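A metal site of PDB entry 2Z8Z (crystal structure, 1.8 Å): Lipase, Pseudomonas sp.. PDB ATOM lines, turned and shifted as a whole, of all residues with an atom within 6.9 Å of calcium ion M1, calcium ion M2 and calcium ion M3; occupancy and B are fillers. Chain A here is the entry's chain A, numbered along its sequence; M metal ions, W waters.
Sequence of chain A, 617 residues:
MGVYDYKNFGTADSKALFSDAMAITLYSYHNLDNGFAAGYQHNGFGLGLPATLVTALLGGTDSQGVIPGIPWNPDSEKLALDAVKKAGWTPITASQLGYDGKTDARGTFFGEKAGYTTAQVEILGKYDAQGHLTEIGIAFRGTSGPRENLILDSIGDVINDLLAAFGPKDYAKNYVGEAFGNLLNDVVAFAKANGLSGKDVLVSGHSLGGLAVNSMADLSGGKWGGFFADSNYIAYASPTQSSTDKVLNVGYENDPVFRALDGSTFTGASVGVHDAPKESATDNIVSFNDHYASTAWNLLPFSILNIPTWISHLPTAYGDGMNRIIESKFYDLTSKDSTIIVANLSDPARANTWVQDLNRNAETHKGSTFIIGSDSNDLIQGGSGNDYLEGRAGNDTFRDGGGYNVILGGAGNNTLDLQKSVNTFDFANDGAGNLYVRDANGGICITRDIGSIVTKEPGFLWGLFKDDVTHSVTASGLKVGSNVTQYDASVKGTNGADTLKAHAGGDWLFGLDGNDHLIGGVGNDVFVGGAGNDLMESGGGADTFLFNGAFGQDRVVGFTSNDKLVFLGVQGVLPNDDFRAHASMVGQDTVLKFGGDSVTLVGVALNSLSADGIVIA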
ATOM      1  N   GLY A 493       5.502  -8.272  -6.216  1.00  0.00           N
ATOM      2  CA  GLY A 493       4.870  -8.226  -4.910  1.00  0.00           C
ATOM      3  C   GLY A 493       3.365  -8.514  -4.898  1.00  0.00           C
ATOM      4  O   GLY A 493       2.847  -9.283  -5.712  1.00  0.00           O
ATOM      5  N   THR A 494       2.684  -7.864  -3.998  1.00  0.00           N
ATOM      6  CA  THR A 494       1.259  -7.962  -3.802  1.00  0.00           C
ATOM      7  C   THR A 494       0.701  -6.566  -3.606  1.00  0.00           C
ATOM      8  O   THR A 494       1.469  -5.617  -3.557  1.00  0.00           O
ATOM      9  CB  THR A 494       0.966  -8.802  -2.558  1.00  0.00           C
ATOM     10  OG1 THR A 494       1.256  -8.069  -1.367  1.00  0.00           O
ATOM     11  CG2 THR A 494       1.699 -10.131  -2.593  1.00  0.00           C
ATOM     12  N   ASN A 495      -0.615  -6.443  -3.479  1.00  0.00           N
ATOM     13  CA  ASN A 495      -1.218  -5.132  -3.194  1.00  0.00           C
ATOM     14  C   ASN A 495      -1.135  -4.706  -1.712  1.00  0.00           C
ATOM     15  O   ASN A 495      -1.654  -3.687  -1.350  1.00  0.00           O
ATOM     16  CB  ASN A 495      -2.647  -5.073  -3.733  1.00  0.00           C
ATOM     17  CG  ASN A 495      -2.677  -4.922  -5.242  1.00  0.00           C
ATOM     18  OD1 ASN A 495      -3.585  -5.443  -5.897  1.00  0.00           O
ATOM     19  ND2 ASN A 495      -1.699  -4.222  -5.798  1.00  0.00           N
ATOM     20  N   GLY A 496      -0.466  -5.507  -0.866  1.00  0.00           N
ATOM     21  CA  GLY A 496      -0.104  -5.108   0.493  1.00  0.00           C
ATOM     22  C   GLY A 496       1.385  -4.711   0.544  1.00  0.00           C
ATOM     23  O   GLY A 496       2.040  -4.631  -0.493  1.00  0.00           O
ATOM     24  N   ALA A 497       1.875  -4.475   1.736  1.00  0.00           N
ATOM     25  CA  ALA A 497       3.288  -4.114   1.985  1.00  0.00           C
ATOM     26  C   ALA A 497       4.199  -5.360   1.841  1.00  0.00           C
ATOM     27  O   ALA A 497       3.980  -6.378   2.528  1.00  0.00           O
ATOM     28  CB  ALA A 497       3.397  -3.560   3.356  1.00  0.00           C
ATOM     29  N   ASP A 498       5.136  -5.298   0.899  1.00  0.00           N
ATOM     30  CA  ASP A 498       6.027  -6.387   0.605  1.00  0.00           C
ATOM     31  C   ASP A 498       7.473  -5.920   0.763  1.00  0.00           C
ATOM     32  O   ASP A 498       7.782  -4.791   0.529  1.00  0.00           O
ATOM     33  CB  ASP A 498       5.926  -6.809  -0.839  1.00  0.00           C
ATOM     34  CG  ASP A 498       4.493  -6.994  -1.336  1.00  0.00           C
ATOM     35  OD1 ASP A 498       3.781  -7.895  -0.838  1.00  0.00           O
ATOM     36  OD2 ASP A 498       4.075  -6.264  -2.274  1.00  0.00           O
ATOM     37  N   LEU A 500      10.719  -6.965  -1.363  1.00  0.00           N
ATOM     38  CA  LEU A 500      11.174  -7.707  -2.499  1.00  0.00           C
ATOM     39  C   LEU A 500      12.682  -7.483  -2.637  1.00  0.00           C
ATOM     40  O   LEU A 500      13.150  -6.369  -2.544  1.00  0.00           O
ATOM     41  CB  LEU A 500      10.519  -7.234  -3.781  1.00  0.00           C
ATOM     42  CG  LEU A 500       9.001  -7.074  -3.804  1.00  0.00           C
ATOM     43  CD1 LEU A 500       8.636  -6.587  -5.164  1.00  0.00           C
ATOM     44  CD2 LEU A 500       8.275  -8.422  -3.422  1.00  0.00           C
ATOM     45  N   PHE A 510       8.519  -5.143  -8.954  1.00  0.00           N
ATOM     46  CA  PHE A 510       7.135  -4.606  -9.043  1.00  0.00           C
ATOM     47  C   PHE A 510       6.442  -4.666  -7.662  1.00  0.00           C
ATOM     48  O   PHE A 510       5.915  -5.727  -7.238  1.00  0.00           O
ATOM     49  CB  PHE A 510       6.356  -5.442 -10.068  1.00  0.00           C
ATOM     50  CG  PHE A 510       6.874  -5.344 -11.473  1.00  0.00           C
ATOM     51  CD1 PHE A 510       6.868  -4.134 -12.167  1.00  0.00           C
ATOM     52  CD2 PHE A 510       7.371  -6.473 -12.153  1.00  0.00           C
ATOM     53  CE1 PHE A 510       7.311  -4.045 -13.459  1.00  0.00           C
ATOM     54  CE2 PHE A 510       7.831  -6.360 -13.480  1.00  0.00           C
ATOM     55  CZ  PHE A 510       7.790  -5.154 -14.125  1.00  0.00           C
ATOM     56  N   GLY A 511       6.483  -3.574  -6.919  1.00  0.00           N
ATOM     57  CA  GLY A 511       5.880  -3.527  -5.620  1.00  0.00           C
ATOM     58  C   GLY A 511       4.357  -3.586  -5.636  1.00  0.00           C
ATOM     59  O   GLY A 511       3.737  -4.046  -4.637  1.00  0.00           O
ATOM     60  N   LEU A 512       3.769  -3.087  -6.731  1.00  0.00           N
ATOM     61  CA  LEU A 512       2.308  -2.892  -6.817  1.00  0.00           C
ATOM     62  C   LEU A 512       1.815  -2.035  -5.614  1.00  0.00           C
ATOM     63  O   LEU A 512       2.575  -1.187  -5.063  1.00  0.00           O
ATOM     64  CB  LEU A 512       1.621  -4.251  -6.841  1.00  0.00           C
ATOM     65  CG  LEU A 512       2.158  -5.268  -7.837  1.00  0.00           C
ATOM     66  CD1 LEU A 512       1.440  -6.610  -7.680  1.00  0.00           C
ATOM     67  CD2 LEU A 512       2.110  -4.754  -9.259  1.00  0.00           C
ATOM     68  N   ASP A 513       0.533  -2.167  -5.239  1.00  0.00           N
ATOM     69  CA  ASP A 513       0.006  -1.315  -4.208  1.00  0.00           C
ATOM     70  C   ASP A 513       0.631  -1.581  -2.848  1.00  0.00           C
ATOM     71  O   ASP A 513       1.266  -2.623  -2.634  1.00  0.00           O
ATOM     72  CB  ASP A 513      -1.522  -1.425  -4.087  1.00  0.00           C
ATOM     73  CG  ASP A 513      -2.288  -1.104  -5.383  1.00  0.00           C
ATOM     74  OD1 ASP A 513      -1.697  -0.623  -6.385  1.00  0.00           O
ATOM     75  OD2 ASP A 513      -3.523  -1.328  -5.348  1.00  0.00           O
ATOM     76  N   GLY A 514       0.466  -0.612  -1.930  1.00  0.00           N
ATOM     77  CA  GLY A 514       0.929  -0.684  -0.585  1.00  0.00           C
ATOM     78  C   GLY A 514       2.355  -0.122  -0.483  1.00  0.00           C
ATOM     79  O   GLY A 514       3.004   0.136  -1.522  1.00  0.00           O
ATOM     80  N   ASN A 515       2.812   0.046   0.765  1.00  0.00           N
ATOM     81  CA  ASN A 515       4.108   0.634   1.080  1.00  0.00           C
ATOM     82  C   ASN A 515       5.168  -0.431   1.071  1.00  0.00           C
ATOM     83  O   ASN A 515       5.292  -1.206   2.016  1.00  0.00           O
ATOM     84  CB  ASN A 515       4.061   1.385   2.395  1.00  0.00           C
ATOM     85  CG  ASN A 515       2.977   2.462   2.446  1.00  0.00           C
ATOM     86  OD1 ASN A 515       2.454   2.909   1.425  1.00  0.00           O
ATOM     87  ND2 ASN A 515       2.608   2.828   3.630  1.00  0.00           N
ATOM     88  N   ASP A 516       5.920  -0.487  -0.015  1.00  0.00           N
ATOM     89  CA  ASP A 516       6.879  -1.569  -0.271  1.00  0.00           C
ATOM     90  C   ASP A 516       8.337  -1.179  -0.003  1.00  0.00           C
ATOM     91  O   ASP A 516       8.665  -0.014   0.117  1.00  0.00           O
ATOM     92  CB  ASP A 516       6.699  -2.074  -1.676  1.00  0.00           C
ATOM     93  CG  ASP A 516       5.254  -2.535  -1.931  1.00  0.00           C
ATOM     94  OD1 ASP A 516       4.752  -3.391  -1.127  1.00  0.00           O
ATOM     95  OD2 ASP A 516       4.672  -2.056  -2.922  1.00  0.00           O
ATOM     96  N   LEU A 518      11.818  -2.157  -1.461  1.00  0.00           N
ATOM     97  CA  LEU A 518      12.430  -2.744  -2.615  1.00  0.00           C
ATOM     98  C   LEU A 518      13.947  -2.717  -2.536  1.00  0.00           C
ATOM     99  O   LEU A 518      14.534  -1.648  -2.575  1.00  0.00           O
ATOM    100  CB  LEU A 518      11.976  -2.033  -3.869  1.00  0.00           C
ATOM    101  CG  LEU A 518      10.680  -2.553  -4.486  1.00  0.00           C
ATOM    102  CD1 LEU A 518       9.640  -2.999  -3.584  1.00  0.00           C
ATOM    103  CD2 LEU A 518      10.150  -1.647  -5.595  1.00  0.00           C
ATOM    104  N   VAL A 528       9.853  -0.417  -9.827  1.00  0.00           N
ATOM    105  CA  VAL A 528       8.504   0.146  -9.977  1.00  0.00           C
ATOM    106  C   VAL A 528       7.733   0.003  -8.666  1.00  0.00           C
ATOM    107  O   VAL A 528       7.021  -1.013  -8.380  1.00  0.00           O
ATOM    108  CB  VAL A 528       7.726  -0.512 -11.130  1.00  0.00           C
ATOM    109  CG1 VAL A 528       6.445   0.301 -11.403  1.00  0.00           C
ATOM    110  CG2 VAL A 528       8.574  -0.639 -12.406  1.00  0.00           C
ATOM    111  N   GLY A 529       7.885   1.013  -7.808  1.00  0.00           N
ATOM    112  CA  GLY A 529       7.255   0.974  -6.482  1.00  0.00           C
ATOM    113  C   GLY A 529       5.748   0.812  -6.573  1.00  0.00           C
ATOM    114  O   GLY A 529       5.117   0.198  -5.718  1.00  0.00           O
ATOM    115  N   GLY A 530       5.168   1.387  -7.611  1.00  0.00           N
ATOM    116  CA  GLY A 530       3.705   1.512  -7.734  1.00  0.00           C
ATOM    117  C   GLY A 530       3.065   2.491  -6.753  1.00  0.00           C
ATOM    118  O   GLY A 530       3.726   3.374  -6.120  1.00  0.00           O
ATOM    119  N   ALA A 531       1.763   2.314  -6.586  1.00  0.00           N
ATOM    120  CA  ALA A 531       1.027   3.040  -5.559  1.00  0.00           C
ATOM    121  C   ALA A 531       1.583   2.751  -4.214  1.00  0.00           C
ATOM    122  O   ALA A 531       2.265   1.721  -4.044  1.00  0.00           O
ATOM    123  CB  ALA A 531      -0.451   2.642  -5.594  1.00  0.00           C
ATOM    124  N   GLY A 532       1.333   3.646  -3.276  1.00  0.00           N
ATOM    125  CA  GLY A 532       1.912   3.573  -1.975  1.00  0.00           C
ATOM    126  C   GLY A 532       3.259   4.281  -1.862  1.00  0.00           C
ATOM    127  O   GLY A 532       3.816   4.716  -2.842  1.00  0.00           O
ATOM    128  N   ASN A 533       3.790   4.276  -0.660  1.00  0.00           N
ATOM    129  CA  ASN A 533       5.012   5.035  -0.274  1.00  0.00           C
ATOM    130  C   ASN A 533       6.065   3.961  -0.145  1.00  0.00           C
ATOM    131  O   ASN A 533       6.096   3.198   0.816  1.00  0.00           O
ATOM    132  CB  ASN A 533       4.768   5.817   1.021  1.00  0.00           C
ATOM    133  CG  ASN A 533       3.534   6.750   0.902  1.00  0.00           C
ATOM    134  OD1 ASN A 533       3.128   7.140  -0.166  1.00  0.00           O
ATOM    135  ND2 ASN A 533       2.974   7.119   2.048  1.00  0.00           N
ATOM    136  N   ASP A 534       6.863   3.869  -1.179  1.00  0.00           N
ATOM    137  CA  ASP A 534       7.792   2.808  -1.328  1.00  0.00           C
ATOM    138  C   ASP A 534       9.196   3.263  -0.983  1.00  0.00           C
ATOM    139  O   ASP A 534       9.583   4.354  -1.395  1.00  0.00           O
ATOM    140  CB  ASP A 534       7.734   2.291  -2.708  1.00  0.00           C
ATOM    141  CG  ASP A 534       6.348   1.832  -3.090  1.00  0.00           C
ATOM    142  OD1 ASP A 534       5.816   0.880  -2.475  1.00  0.00           O
ATOM    143  OD2 ASP A 534       5.777   2.461  -3.973  1.00  0.00           O
ATOM    144  N   MET A 536      13.030   2.382  -1.745  1.00  0.00           N
ATOM    145  CA  MET A 536      13.685   1.707  -2.822  1.00  0.00           C
ATOM    146  C   MET A 536      15.158   1.900  -2.804  1.00  0.00           C
ATOM    147  O   MET A 536      15.627   3.029  -2.844  1.00  0.00           O
ATOM    148  CB  MET A 536      13.079   2.106  -4.153  1.00  0.00           C
ATOM    149  CG  MET A 536      11.566   1.929  -4.204  1.00  0.00           C
ATOM    150  SD  MET A 536      10.870   2.332  -5.777  1.00  0.00           S
ATOM    151  CE  MET A 536      10.626   4.050  -5.592  1.00  0.00           C
ATOM    152  N   PHE A 547       8.241   5.973 -12.209  1.00  0.00           N
ATOM    153  CA  PHE A 547       7.153   6.583 -11.466  1.00  0.00           C
ATOM    154  C   PHE A 547       6.059   6.962 -12.459  1.00  0.00           C
ATOM    155  O   PHE A 547       6.343   7.637 -13.423  1.00  0.00           O
ATOM    156  CB  PHE A 547       7.628   7.816 -10.728  1.00  0.00           C
ATOM    157  CG  PHE A 547       8.824   7.554  -9.863  1.00  0.00           C
ATOM    158  CD1 PHE A 547       8.669   7.099  -8.578  1.00  0.00           C
ATOM    159  CD2 PHE A 547      10.103   7.812 -10.340  1.00  0.00           C
ATOM    160  CE1 PHE A 547       9.813   6.846  -7.774  1.00  0.00           C
ATOM    161  CE2 PHE A 547      11.196   7.503  -9.565  1.00  0.00           C
ATOM    162  CZ  PHE A 547      11.053   7.062  -8.287  1.00  0.00           C
ATOM    163  N   ALA A 550      -0.473   8.145  -9.676  1.00  0.00           N
ATOM    164  CA  ALA A 550      -0.457   8.733  -8.325  1.00  0.00           C
ATOM    165  C   ALA A 550       0.486   7.857  -7.514  1.00  0.00           C
ATOM    166  O   ALA A 550       0.074   6.917  -6.800  1.00  0.00           O
ATOM    167  CB  ALA A 550      -1.827   8.762  -7.725  1.00  0.00           C
ATOM    168  N   PHE A 551       1.767   8.118  -7.677  1.00  0.00           N
ATOM    169  CA  PHE A 551       2.798   7.135  -7.285  1.00  0.00           C
ATOM    170  C   PHE A 551       3.198   7.196  -5.818  1.00  0.00           C
ATOM    171  O   PHE A 551       3.958   6.368  -5.329  1.00  0.00           O
ATOM    172  CB  PHE A 551       3.989   7.218  -8.207  1.00  0.00           C
ATOM    173  CG  PHE A 551       4.729   8.534  -8.161  1.00  0.00           C
ATOM    174  CD1 PHE A 551       5.648   8.781  -7.170  1.00  0.00           C
ATOM    175  CD2 PHE A 551       4.531   9.479  -9.146  1.00  0.00           C
ATOM    176  CE1 PHE A 551       6.360  10.048  -7.131  1.00  0.00           C
ATOM    177  CE2 PHE A 551       5.217  10.669  -9.140  1.00  0.00           C
ATOM    178  CZ  PHE A 551       6.122  10.977  -8.125  1.00  0.00           C
ATOM    179  N   GLY A 552       2.648   8.171  -5.094  1.00  0.00           N
ATOM    180  CA  GLY A 552       2.879   8.279  -3.655  1.00  0.00           C
ATOM    181  C   GLY A 552       4.105   9.050  -3.236  1.00  0.00           C
ATOM    182  O   GLY A 552       4.588   9.945  -3.989  1.00  0.00           O
ATOM    183  N   GLN A 553       4.522   8.805  -1.987  1.00  0.00           N
ATOM    184  CA  GLN A 553       5.656   9.519  -1.360  1.00  0.00           C
ATOM    185  C   GLN A 553       6.738   8.445  -1.214  1.00  0.00           C
ATOM    186  O   GLN A 553       6.718   7.637  -0.256  1.00  0.00           O
ATOM    187  CB  GLN A 553       5.341  10.139  -0.009  1.00  0.00           C
ATOM    188  CG  GLN A 553       3.937  10.699   0.111  1.00  0.00           C
ATOM    189  CD  GLN A 553       3.640  11.693  -0.925  1.00  0.00           C
ATOM    190  OE1 GLN A 553       2.561  11.674  -1.528  1.00  0.00           O
ATOM    191  NE2 GLN A 553       4.557  12.584  -1.152  1.00  0.00           N
ATOM    192  N   ASP A 554       7.654   8.451  -2.168  1.00  0.00           N
ATOM    193  CA  ASP A 554       8.685   7.416  -2.241  1.00  0.00           C
ATOM    194  C   ASP A 554      10.021   7.951  -1.724  1.00  0.00           C
ATOM    195  O   ASP A 554      10.240   9.151  -1.759  1.00  0.00           O
ATOM    196  CB  ASP A 554       8.863   6.939  -3.674  1.00  0.00           C
ATOM    197  CG  ASP A 554       7.636   6.248  -4.260  1.00  0.00           C
ATOM    198  OD1 ASP A 554       6.823   5.577  -3.500  1.00  0.00           O
ATOM    199  OD2 ASP A 554       7.536   6.347  -5.515  1.00  0.00           O
ATOM    200  N   SER A 598       5.662  12.470  -4.557  1.00  0.00           N
ATOM    201  CA  SER A 598       7.020  12.958  -4.325  1.00  0.00           C
ATOM    202  C   SER A 598       8.002  11.802  -4.283  1.00  0.00           C
ATOM    203  O   SER A 598       7.640  10.668  -3.976  1.00  0.00           O
ATOM    204  CB  SER A 598       7.105  13.757  -3.038  1.00  0.00           C
ATOM    205  OG  SER A 598       7.078  12.945  -1.880  1.00  0.00           O
HETATM  206 CA    CA M   1       5.099   4.551  -4.801  1.00  0.00          CA
HETATM  207 CA    CA M   2       3.915   0.105  -3.668  1.00  0.00          CA
HETATM  208 CA    CA M   3       3.017  -4.182  -2.569  1.00  0.00          CA
HETATM  209  O   HOH W   1       6.475   4.361  -6.776  1.00  0.00           O
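Within 4 Å of calcium ion M2: Leu 512, Asp 513, Gly 514, Asp 516, Gly 529, Gly 530, Ala 531 and Asp 534. The nearest printed residue that does not touch calcium ion M2 is Gly 511 (4.2 Å).
Water W1 bridges OD2 of Asp 554 (2.6 Å) and N of Gly 530 (3.4 Å).
N of Gly 511 sits at hydrogen-bond distance from O of Val 528. The side-chain hydroxyl (OG1) of Thr 494 sits at hydrogen-bond distance from the backbone NH (N) of Gly 496, 3.1 Å away. ND2 of Asn 495 sits close to N of Asp 513 (3.1 Å). The backbone NH (N) of Asp 554 sits at hydrogen-bond distance from the backbone carbonyl oxygen (O) of Ser 598, at 2.9 Å.
Calcium ion M3 is bound by O of Gly 511 (2.2 Å), O of Thr 494 (2.3 Å), O of Gly 496 (2.3 Å), O of Asp 513 (2.3 Å), OD2 of Asp 498 (2.4 Å), OD1 of Asp 516 (2.4 Å) and OD2 of Asp 516 (2.7 Å).
Six residues have an atom within 4 Å of calcium ion M1: Gly 530, Ala 531, Gly 532, Asp 534, Phe 551 and Asp 554. The nearest printed residue that does not touch calcium ion M1 is Gly 529 (4.2 Å).
Calcium ion M2 is bound by O of Leu 512 (2.3 Å), O of Gly 514 (2.3 Å), O of Ala 531 (2.3 Å), OD1 of Asp 534 (2.4 Å), O of Gly 529 (2.4 Å) and OD2 of Asp 516 (2.4 Å). Calcium ion M2 has six donor atoms within binding distance. Slightly farther from calcium ion M2 lies the side-chain carboxylate (OD2) of Asp 534 (3.0 Å).
Within 4 Å of calcium ion M3: Thr 494, Gly 496, Asp 498, Gly 511, Leu 512, Asp 513 and Asp 516. Along chain A the residues within 4 Å of calcium ion M3 span positions 494 to 516.
Calcium ion M1 is bound by O of Phe 551, O of Gly 530, O of Gly 532, OD2 of Asp 534, OD1 of Asp 554 and water W1. Calcium ion M1 has six donor atoms within binding distance. Slightly farther from calcium ion M1 lies OD2 of Asp 554 (3.1 Å).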
